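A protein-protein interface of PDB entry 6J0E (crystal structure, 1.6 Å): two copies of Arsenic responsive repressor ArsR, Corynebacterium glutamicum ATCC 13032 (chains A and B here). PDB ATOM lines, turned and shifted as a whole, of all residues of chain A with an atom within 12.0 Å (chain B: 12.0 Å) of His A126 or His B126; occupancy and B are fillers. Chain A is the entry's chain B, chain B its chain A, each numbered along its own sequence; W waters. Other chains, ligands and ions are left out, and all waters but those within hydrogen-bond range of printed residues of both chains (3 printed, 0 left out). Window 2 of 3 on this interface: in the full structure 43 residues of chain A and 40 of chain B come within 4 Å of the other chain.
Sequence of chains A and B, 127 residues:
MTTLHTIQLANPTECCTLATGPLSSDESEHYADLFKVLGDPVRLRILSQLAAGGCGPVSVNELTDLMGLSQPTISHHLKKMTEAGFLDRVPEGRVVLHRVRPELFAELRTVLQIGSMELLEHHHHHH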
ATOM      1  N   THR A   3     -27.741  15.823   8.389  1.00  0.00           N
ATOM      2  CA  THR A   3     -29.138  15.370   8.159  1.00  0.00           C
ATOM      3  C   THR A   3     -29.343  13.914   8.699  1.00  0.00           C
ATOM      4  O   THR A   3     -28.478  13.085   8.484  1.00  0.00           O
ATOM      5  CB  THR A   3     -29.500  15.542   6.655  1.00  0.00           C
ATOM      6  OG1 THR A   3     -30.839  15.146   6.457  1.00  0.00           O
ATOM      7  CG2 THR A   3     -28.527  14.761   5.672  1.00  0.00           C
ATOM      8  N   LEU A 120     -26.455  10.335  11.199  1.00  0.00           N
ATOM      9  CA  LEU A 120     -26.407  11.733  10.648  1.00  0.00           C
ATOM     10  C   LEU A 120     -25.374  11.756   9.502  1.00  0.00           C
ATOM     11  O   LEU A 120     -24.372  11.106   9.577  1.00  0.00           O
ATOM     12  CB  LEU A 120     -25.988  12.710  11.718  1.00  0.00           C
ATOM     13  CG  LEU A 120     -26.909  12.844  12.924  1.00  0.00           C
ATOM     14  CD1 LEU A 120     -26.322  13.786  14.040  1.00  0.00           C
ATOM     15  CD2 LEU A 120     -28.288  13.346  12.487  1.00  0.00           C
ATOM     16  N   GLU A 121     -25.763  12.373   8.410  1.00  0.00           N
ATOM     17  CA  GLU A 121     -24.907  12.558   7.254  1.00  0.00           C
ATOM     18  C   GLU A 121     -24.408  14.012   7.260  1.00  0.00           C
ATOM     19  O   GLU A 121     -25.203  14.927   7.435  1.00  0.00           O
ATOM     20  CB  GLU A 121     -25.642  12.341   5.956  1.00  0.00           C
ATOM     21  CG  GLU A 121     -26.289  10.921   5.675  1.00  0.00           C
ATOM     22  CD  GLU A 121     -25.287   9.857   5.309  1.00  0.00           C
ATOM     23  OE1 GLU A 121     -24.082  10.040   5.358  1.00  0.00           O
ATOM     24  OE2 GLU A 121     -25.677   8.728   5.034  1.00  0.00           O
ATOM     25  N   HIS A 122     -23.097  14.215   7.121  1.00  0.00           N
ATOM     26  CA  HIS A 122     -22.623  15.605   7.081  1.00  0.00           C
ATOM     27  C   HIS A 122     -21.656  15.689   5.927  1.00  0.00           C
ATOM     28  O   HIS A 122     -20.715  15.025   5.952  1.00  0.00           O
ATOM     29  CB  HIS A 122     -21.910  15.908   8.350  1.00  0.00           C
ATOM     30  CG  HIS A 122     -21.776  17.373   8.585  1.00  0.00           C
ATOM     31  ND1 HIS A 122     -21.843  17.933   9.837  1.00  0.00           N
ATOM     32  CD2 HIS A 122     -21.673  18.399   7.709  1.00  0.00           C
ATOM     33  CE1 HIS A 122     -21.669  19.246   9.731  1.00  0.00           C
ATOM     34  NE2 HIS A 122     -21.596  19.572   8.444  1.00  0.00           N
ATOM     35  N   HIS A 123     -21.957  16.516   4.900  1.00  0.00           N
ATOM     36  CA  HIS A 123     -20.945  16.724   3.785  1.00  0.00           C
ATOM     37  C   HIS A 123     -20.154  17.973   4.039  1.00  0.00           C
ATOM     38  O   HIS A 123     -20.690  18.950   4.574  1.00  0.00           O
ATOM     39  CB  HIS A 123     -21.710  16.904   2.480  1.00  0.00           C
ATOM     40  CG  HIS A 123     -22.398  15.652   2.008  1.00  0.00           C
ATOM     41  ND1 HIS A 123     -21.822  14.783   1.133  1.00  0.00           N
ATOM     42  CD2 HIS A 123     -23.568  15.065   2.404  1.00  0.00           C
ATOM     43  CE1 HIS A 123     -22.604  13.716   0.981  1.00  0.00           C
ATOM     44  NE2 HIS A 123     -23.655  13.856   1.744  1.00  0.00           N
ATOM     45  N   HIS A 124     -18.878  17.874   3.710  1.00  0.00           N
ATOM     46  CA  HIS A 124     -17.884  18.933   3.923  1.00  0.00           C
ATOM     47  C   HIS A 124     -17.194  19.126   2.589  1.00  0.00           C
ATOM     48  O   HIS A 124     -16.999  18.248   1.837  1.00  0.00           O
ATOM     49  CB  HIS A 124     -16.832  18.597   4.918  1.00  0.00           C
ATOM     50  CG  HIS A 124     -17.356  18.239   6.287  1.00  0.00           C
ATOM     51  ND1 HIS A 124     -17.657  19.175   7.262  1.00  0.00           N
ATOM     52  CD2 HIS A 124     -17.730  17.023   6.791  1.00  0.00           C
ATOM     53  CE1 HIS A 124     -18.131  18.544   8.329  1.00  0.00           C
ATOM     54  NE2 HIS A 124     -18.227  17.249   8.052  1.00  0.00           N
ATOM     55  N   HIS A 125     -17.012  20.428   2.267  1.00  0.00           N
ATOM     56  CA  HIS A 125     -16.175  20.779   1.126  1.00  0.00           C
ATOM     57  C   HIS A 125     -14.899  21.512   1.544  1.00  0.00           C
ATOM     58  O   HIS A 125     -14.786  22.123   2.617  1.00  0.00           O
ATOM     59  CB  HIS A 125     -17.049  21.649   0.226  1.00  0.00           C
ATOM     60  CG  HIS A 125     -18.140  20.852  -0.382  1.00  0.00           C
ATOM     61  ND1 HIS A 125     -17.910  19.939  -1.407  1.00  0.00           N
ATOM     62  CD2 HIS A 125     -19.437  20.671   0.016  1.00  0.00           C
ATOM     63  CE1 HIS A 125     -19.076  19.326  -1.675  1.00  0.00           C
ATOM     64  NE2 HIS A 125     -19.992  19.753  -0.827  1.00  0.00           N
ATOM     65  N   HIS A 126     -13.960  21.335   0.688  1.00  0.00           N
ATOM     66  CA  HIS A 126     -12.574  21.792   0.978  1.00  0.00           C
ATOM     67  C   HIS A 126     -12.058  22.577  -0.233  1.00  0.00           C
ATOM     68  O   HIS A 126     -12.544  22.429  -1.322  1.00  0.00           O
ATOM     69  CB  HIS A 126     -11.714  20.597   1.346  1.00  0.00           C
ATOM     70  CG  HIS A 126     -12.067  19.975   2.636  1.00  0.00           C
ATOM     71  ND1 HIS A 126     -11.597  20.445   3.862  1.00  0.00           N
ATOM     72  CD2 HIS A 126     -12.925  18.969   2.920  1.00  0.00           C
ATOM     73  CE1 HIS A 126     -12.175  19.771   4.819  1.00  0.00           C
ATOM     74  NE2 HIS A 126     -12.887  18.801   4.270  1.00  0.00           N
ATOM     75  N   HIS A 127     -11.136  23.495  -0.039  1.00  0.00           N
ATOM     76  CA  HIS A 127     -10.717  24.249  -1.271  1.00  0.00           C
ATOM     77  C   HIS A 127      -9.311  24.593  -1.085  1.00  0.00           C
ATOM     78  O   HIS A 127      -8.842  24.322  -0.001  1.00  0.00           O
ATOM     79  CB  HIS A 127     -11.559  25.522  -1.427  1.00  0.00           C
ATOM     80  CG  HIS A 127     -11.244  26.547  -0.400  1.00  0.00           C
ATOM     81  ND1 HIS A 127     -11.732  26.507   0.900  1.00  0.00           N
ATOM     82  CD2 HIS A 127     -10.369  27.571  -0.455  1.00  0.00           C
ATOM     83  CE1 HIS A 127     -11.188  27.482   1.593  1.00  0.00           C
ATOM     84  NE2 HIS A 127     -10.339  28.123   0.796  1.00  0.00           N
ATOM     85  OXT HIS A 127      -8.691  25.121  -2.031  1.00  0.00           O
ATOM     86  N   THR B   2     -12.563  13.316  -4.949  1.00  0.00           N
ATOM     87  CA  THR B   2     -12.098  12.358  -3.961  1.00  0.00           C
ATOM     88  C   THR B   2     -12.910  12.653  -2.723  1.00  0.00           C
ATOM     89  O   THR B   2     -13.314  13.798  -2.527  1.00  0.00           O
ATOM     90  CB  THR B   2     -10.626  12.549  -3.669  1.00  0.00           C
ATOM     91  OG1 THR B   2     -10.220  11.784  -2.590  1.00  0.00           O
ATOM     92  CG2 THR B   2     -10.225  13.862  -3.456  1.00  0.00           C
ATOM     93  N   THR B   3     -13.113  11.623  -1.927  1.00  0.00           N
ATOM     94  CA  THR B   3     -13.862  11.837  -0.677  1.00  0.00           C
ATOM     95  C   THR B   3     -13.190  11.056   0.389  1.00  0.00           C
ATOM     96  O   THR B   3     -13.118   9.840   0.249  1.00  0.00           O
ATOM     97  CB  THR B   3     -15.327  11.365  -0.767  1.00  0.00           C
ATOM     98  OG1 THR B   3     -15.952  11.963  -1.899  1.00  0.00           O
ATOM     99  CG2 THR B   3     -16.175  11.756   0.510  1.00  0.00           C
ATOM    100  N   LEU B   4     -12.906  11.733   1.496  1.00  0.00           N
ATOM    101  CA  LEU B   4     -12.463  11.126   2.667  1.00  0.00           C
ATOM    102  C   LEU B   4     -13.715  10.915   3.561  1.00  0.00           C
ATOM    103  O   LEU B   4     -14.339  11.825   3.969  1.00  0.00           O
ATOM    104  CB  LEU B   4     -11.361  11.943   3.316  1.00  0.00           C
ATOM    105  CG  LEU B   4     -10.894  11.590   4.752  1.00  0.00           C
ATOM    106  CD1 LEU B   4     -10.300  10.179   4.763  1.00  0.00           C
ATOM    107  CD2 LEU B   4      -9.930  12.654   5.287  1.00  0.00           C
ATOM    108  N   HIS B   5     -14.008   9.652   3.876  1.00  0.00           N
ATOM    109  CA  HIS B   5     -15.070   9.310   4.760  1.00  0.00           C
ATOM    110  C   HIS B   5     -14.591   9.064   6.212  1.00  0.00           C
ATOM    111  O   HIS B   5     -13.565   8.345   6.445  1.00  0.00           O
ATOM    112  CB  HIS B   5     -15.775   8.067   4.229  1.00  0.00           C
ATOM    113  CG  HIS B   5     -16.405   8.239   2.920  1.00  0.00           C
ATOM    114  ND1 HIS B   5     -17.695   8.629   2.775  1.00  0.00           N
ATOM    115  CD2 HIS B   5     -15.921   7.995   1.669  1.00  0.00           C
ATOM    116  CE1 HIS B   5     -17.956   8.707   1.472  1.00  0.00           C
ATOM    117  NE2 HIS B   5     -16.900   8.313   0.792  1.00  0.00           N
ATOM    118  N   THR B   6     -15.316   9.621   7.166  1.00  0.00           N
ATOM    119  CA  THR B   6     -15.003   9.251   8.577  1.00  0.00           C
ATOM    120  C   THR B   6     -16.353   8.955   9.214  1.00  0.00           C
ATOM    121  O   THR B   6     -17.312   9.640   8.997  1.00  0.00           O
ATOM    122  CB  THR B   6     -14.251  10.361   9.257  1.00  0.00           C
ATOM    123  OG1 THR B   6     -15.112  11.503   9.436  1.00  0.00           O
ATOM    124  CG2 THR B   6     -12.928  10.782   8.368  1.00  0.00           C
ATOM    125  N   GLN B   8     -17.820   9.303  12.957  1.00  0.00           N
ATOM    126  CA  GLN B   8     -17.592   9.811  14.295  1.00  0.00           C
ATOM    127  C   GLN B   8     -18.869   9.803  15.193  1.00  0.00           C
ATOM    128  O   GLN B   8     -20.013   9.498  14.759  1.00  0.00           O
ATOM    129  CB  GLN B   8     -17.046  11.243  14.174  1.00  0.00           C
ATOM    130  CG  GLN B   8     -15.716  11.180  13.471  1.00  0.00           C
ATOM    131  CD  GLN B   8     -15.204  12.484  13.111  1.00  0.00           C
ATOM    132  OE1 GLN B   8     -14.790  12.707  11.956  1.00  0.00           O
ATOM    133  NE2 GLN B   8     -15.293  13.414  14.030  1.00  0.00           N
ATOM    134  N   HIS B 122     -21.685  10.360   9.800  1.00  0.00           N
ATOM    135  CA  HIS B 122     -20.874   9.935   8.660  1.00  0.00           C
ATOM    136  C   HIS B 122     -20.496  11.298   8.000  1.00  0.00           C
ATOM    137  O   HIS B 122     -21.396  11.987   7.542  1.00  0.00           O
ATOM    138  CB  HIS B 122     -21.726   9.109   7.666  1.00  0.00           C
ATOM    139  CG  HIS B 122     -20.983   8.683   6.457  1.00  0.00           C
ATOM    140  ND1 HIS B 122     -21.522   7.884   5.496  1.00  0.00           N
ATOM    141  CD2 HIS B 122     -19.740   9.003   6.013  1.00  0.00           C
ATOM    142  CE1 HIS B 122     -20.644   7.732   4.489  1.00  0.00           C
ATOM    143  NE2 HIS B 122     -19.576   8.457   4.761  1.00  0.00           N
ATOM    144  N   HIS B 123     -19.225  11.698   8.114  1.00  0.00           N
ATOM    145  CA  HIS B 123     -18.683  12.920   7.471  1.00  0.00           C
ATOM    146  C   HIS B 123     -18.078  12.525   6.105  1.00  0.00           C
ATOM    147  O   HIS B 123     -17.262  11.578   6.009  1.00  0.00           O
ATOM    148  CB  HIS B 123     -17.538  13.398   8.343  1.00  0.00           C
ATOM    149  CG  HIS B 123     -17.994  13.906   9.659  1.00  0.00           C
ATOM    150  ND1 HIS B 123     -18.576  15.166   9.863  1.00  0.00           N
ATOM    151  CD2 HIS B 123     -18.076  13.251  10.851  1.00  0.00           C
ATOM    152  CE1 HIS B 123     -18.961  15.247  11.135  1.00  0.00           C
ATOM    153  NE2 HIS B 123     -18.644  14.118  11.745  1.00  0.00           N
ATOM    154  N   HIS B 124     -18.509  13.282   5.093  1.00  0.00           N
ATOM    155  CA  HIS B 124     -18.059  13.048   3.807  1.00  0.00           C
ATOM    156  C   HIS B 124     -17.123  14.281   3.479  1.00  0.00           C
ATOM    157  O   HIS B 124     -17.661  15.404   3.316  1.00  0.00           O
ATOM    158  CB  HIS B 124     -19.207  13.097   2.823  1.00  0.00           C
ATOM    159  CG  HIS B 124     -20.340  12.077   3.055  1.00  0.00           C
ATOM    160  ND1 HIS B 124     -20.582  11.020   2.155  1.00  0.00           N
ATOM    161  CD2 HIS B 124     -21.264  11.988   4.063  1.00  0.00           C
ATOM    162  CE1 HIS B 124     -21.644  10.357   2.633  1.00  0.00           C
ATOM    163  NE2 HIS B 124     -22.044  10.904   3.776  1.00  0.00           N
ATOM    164  N   HIS B 125     -15.880  14.059   3.408  1.00  0.00           N
ATOM    165  CA  HIS B 125     -14.923  15.183   3.172  1.00  0.00           C
ATOM    166  C   HIS B 125     -14.557  15.169   1.702  1.00  0.00           C
ATOM    167  O   HIS B 125     -13.731  14.462   1.269  1.00  0.00           O
ATOM    168  CB  HIS B 125     -13.731  15.087   4.094  1.00  0.00           C
ATOM    169  CG  HIS B 125     -14.066  15.515   5.507  1.00  0.00           C
ATOM    170  ND1 HIS B 125     -14.156  16.852   5.875  1.00  0.00           N
ATOM    171  CD2 HIS B 125     -14.410  14.778   6.609  1.00  0.00           C
ATOM    172  CE1 HIS B 125     -14.508  16.893   7.164  1.00  0.00           C
ATOM    173  NE2 HIS B 125     -14.691  15.657   7.609  1.00  0.00           N
ATOM    174  N   HIS B 126     -15.235  16.031   0.936  1.00  0.00           N
ATOM    175  CA  HIS B 126     -15.021  16.094  -0.513  1.00  0.00           C
ATOM    176  C   HIS B 126     -13.834  16.918  -0.793  1.00  0.00           C
ATOM    177  O   HIS B 126     -13.729  18.039  -0.225  1.00  0.00           O
ATOM    178  CB  HIS B 126     -16.231  16.724  -1.162  1.00  0.00           C
ATOM    179  CG  HIS B 126     -17.533  15.979  -0.939  1.00  0.00           C
ATOM    180  ND1 HIS B 126     -17.884  14.916  -1.743  1.00  0.00           N
ATOM    181  CD2 HIS B 126     -18.551  16.129  -0.034  1.00  0.00           C
ATOM    182  CE1 HIS B 126     -19.015  14.399  -1.301  1.00  0.00           C
ATOM    183  NE2 HIS B 126     -19.509  15.166  -0.359  1.00  0.00           N
ATOM    184  N   HIS B 127     -12.920  16.405  -1.604  1.00  0.00           N
ATOM    185  CA  HIS B 127     -11.726  17.196  -1.916  1.00  0.00           C
ATOM    186  C   HIS B 127     -11.206  16.806  -3.264  1.00  0.00           C
ATOM    187  O   HIS B 127     -11.929  16.147  -3.912  1.00  0.00           O
ATOM    188  CB  HIS B 127     -10.610  17.049  -0.875  1.00  0.00           C
ATOM    189  CG  HIS B 127     -10.108  15.651  -0.689  1.00  0.00           C
ATOM    190  ND1 HIS B 127      -8.815  15.268  -0.848  1.00  0.00           N
ATOM    191  CD2 HIS B 127     -10.781  14.548  -0.283  1.00  0.00           C
ATOM    192  CE1 HIS B 127      -8.674  13.996  -0.534  1.00  0.00           C
ATOM    193  NE2 HIS B 127      -9.861  13.525  -0.177  1.00  0.00           N
ATOM    194  OXT HIS B 127     -10.070  17.098  -3.603  1.00  0.00           O
HETATM  195  O   HOH W   1     -23.931   6.786   5.369  1.00  0.00           O
HETATM  196  O   HOH W   2     -23.849   8.009   3.000  1.00  0.00           O
HETATM  197  O   HOH W   3     -14.972  20.140  -1.912  1.00  0.00           O
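Water W1 bridges OE2 of Glu A121 and ND1 of His B122. Water W2 lies within hydrogen-bond range of OE2 of Glu A121 (2.8 Å), ND1 of His B122 (3.4 Å) and NE2 of His B124 (3.5 Å). Water W3 lies within hydrogen-bond range of the backbone carbonyl oxygen of His B126, a ring nitrogen (ND1) of His A125 and the backbone NH of His A126.
N of His A126 sits close to O of His B126. N of His B122 is in hydrogen-bond range of O of Leu A120 (2.8 Å). The backbone NH of His A122 sits at hydrogen-bond distance from the backbone carbonyl oxygen of His B122. The side-chain carboxylate (OE1) of Glu A121 lies within hydrogen-bond range of a ring nitrogen (NE2) of His B124 (2.7 Å). NE2 of His A124 sits at hydrogen-bond distance from ND1 of His B123 (2.8 Å). OE1 of Glu A121 lies within hydrogen-bond range of ND1 of His B122 (3.3 Å). O of His B124 is in hydrogen-bond range of N of His A124 (2.8 Å). NE2 of His B126 sits at hydrogen-bond distance from ND1 of His A123, 2.8 Å away. O of His A122 is in hydrogen-bond range of N of His B124, 2.9 Å away. The backbone carbonyl oxygen (O) of His A124 lies within hydrogen-bond range of the backbone NH (N) of His B126, at 3.0 Å. NE2 of His A126 is in hydrogen-bond range of ND1 of His B125 (2.8 Å).
Of chain A, only His A123 (2.8 Å), His A124 (3.0 Å), His A125 (3.6 Å) and His A126 (3.4 Å) come within 4 Å of His B126. His A123 touches just these residues of chain B: His B124 and His B126. Of chain B, only His B123 (2.8 Å), His B124 (2.8 Å), His B125 (3.2 Å) and His B126 (3.0 Å) come within 4 Å of His A124. His A125 touches one residue of chain B. No residue of chain B comes within 4 Å of His A127. No residue of chain A comes within 4 Å of Thr B2. Thr B3 touches none of the printed residues of chain A. His B124 touches just these residues of chain A: Glu A121, His A122, His A123 and His A124. Of the printed residues of chain B, Leu A120 touches His B122 (2.8 Å). Of the printed residues of chain A, His B122 touches Leu A120 (2.8 Å), Glu A121 (3.3 Å) and His A122 (2.8 Å). Gln B8 touches none of the printed residues of chain A. The nearest residue of chain B that does not touch His A126 is His B127 (4.3 Å). The nearest printed residue of chain B that does not touch His A122 is His B125 (5.5 Å).
Among the printed residues, pairs that only touch across the chains: His A122 with His B123, His A123 with His B124, His A124 with His B125 and His A125 with His B126.
His A122 touches His B123, but with the chains exchanged His A123 does not touch His B122 (5.3 Å). His A122 touches His B124, but with the chains exchanged His A124 does not touch His B122 (6.2 Å). His A123 touches His B124, and with the chains exchanged His A124 touches His B123. His A123 touches His B126, but with the chains exchanged His A126 does not touch His B123 (8.2 Å). 7 positions are printed for both chains. Of the 15 pairs that touch across the chains among the printed residues, 7 have their exchanged pair printed and touching as well.
The backbone NH (N) of Glu A121 lies within hydrogen-bond range of the backbone carbonyl oxygen (O) of Thr A3, 2.8 Å away. A ring nitrogen (ND1) of His B5 is in hydrogen-bond range of a ring nitrogen (NE2) of His B122 (2.7 Å). O of Thr B6 lies within hydrogen-bond range of N of His B123, 2.9 Å away. The backbone carbonyl oxygen of Leu B4 is in hydrogen-bond range of the backbone NH of His B125, 2.8 Å away.
Of the 9 printed residues of chain A, 7 touch a printed residue of chain B. Of the 12 printed residues of chain B, 5 touch a printed residue of chain A. Printed residues of chain B that touch a printed residue of chain A: His B122, His B123, His B124, His B125 and His B126. Hydrophobic or aromatic side chains of chain B that line the printed part of chain A: His B122, His B123, His B124, His B125 and His B126. Along chain B the printed residues that touch a printed residue of chain A span positions 122 to 126. Among the printed residues, 15 pairs touch across the chains. Among the printed residues, no Asp or Glu carboxylate lies within 4 Å of a Lys or Arg side-chain nitrogen of the other chain.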
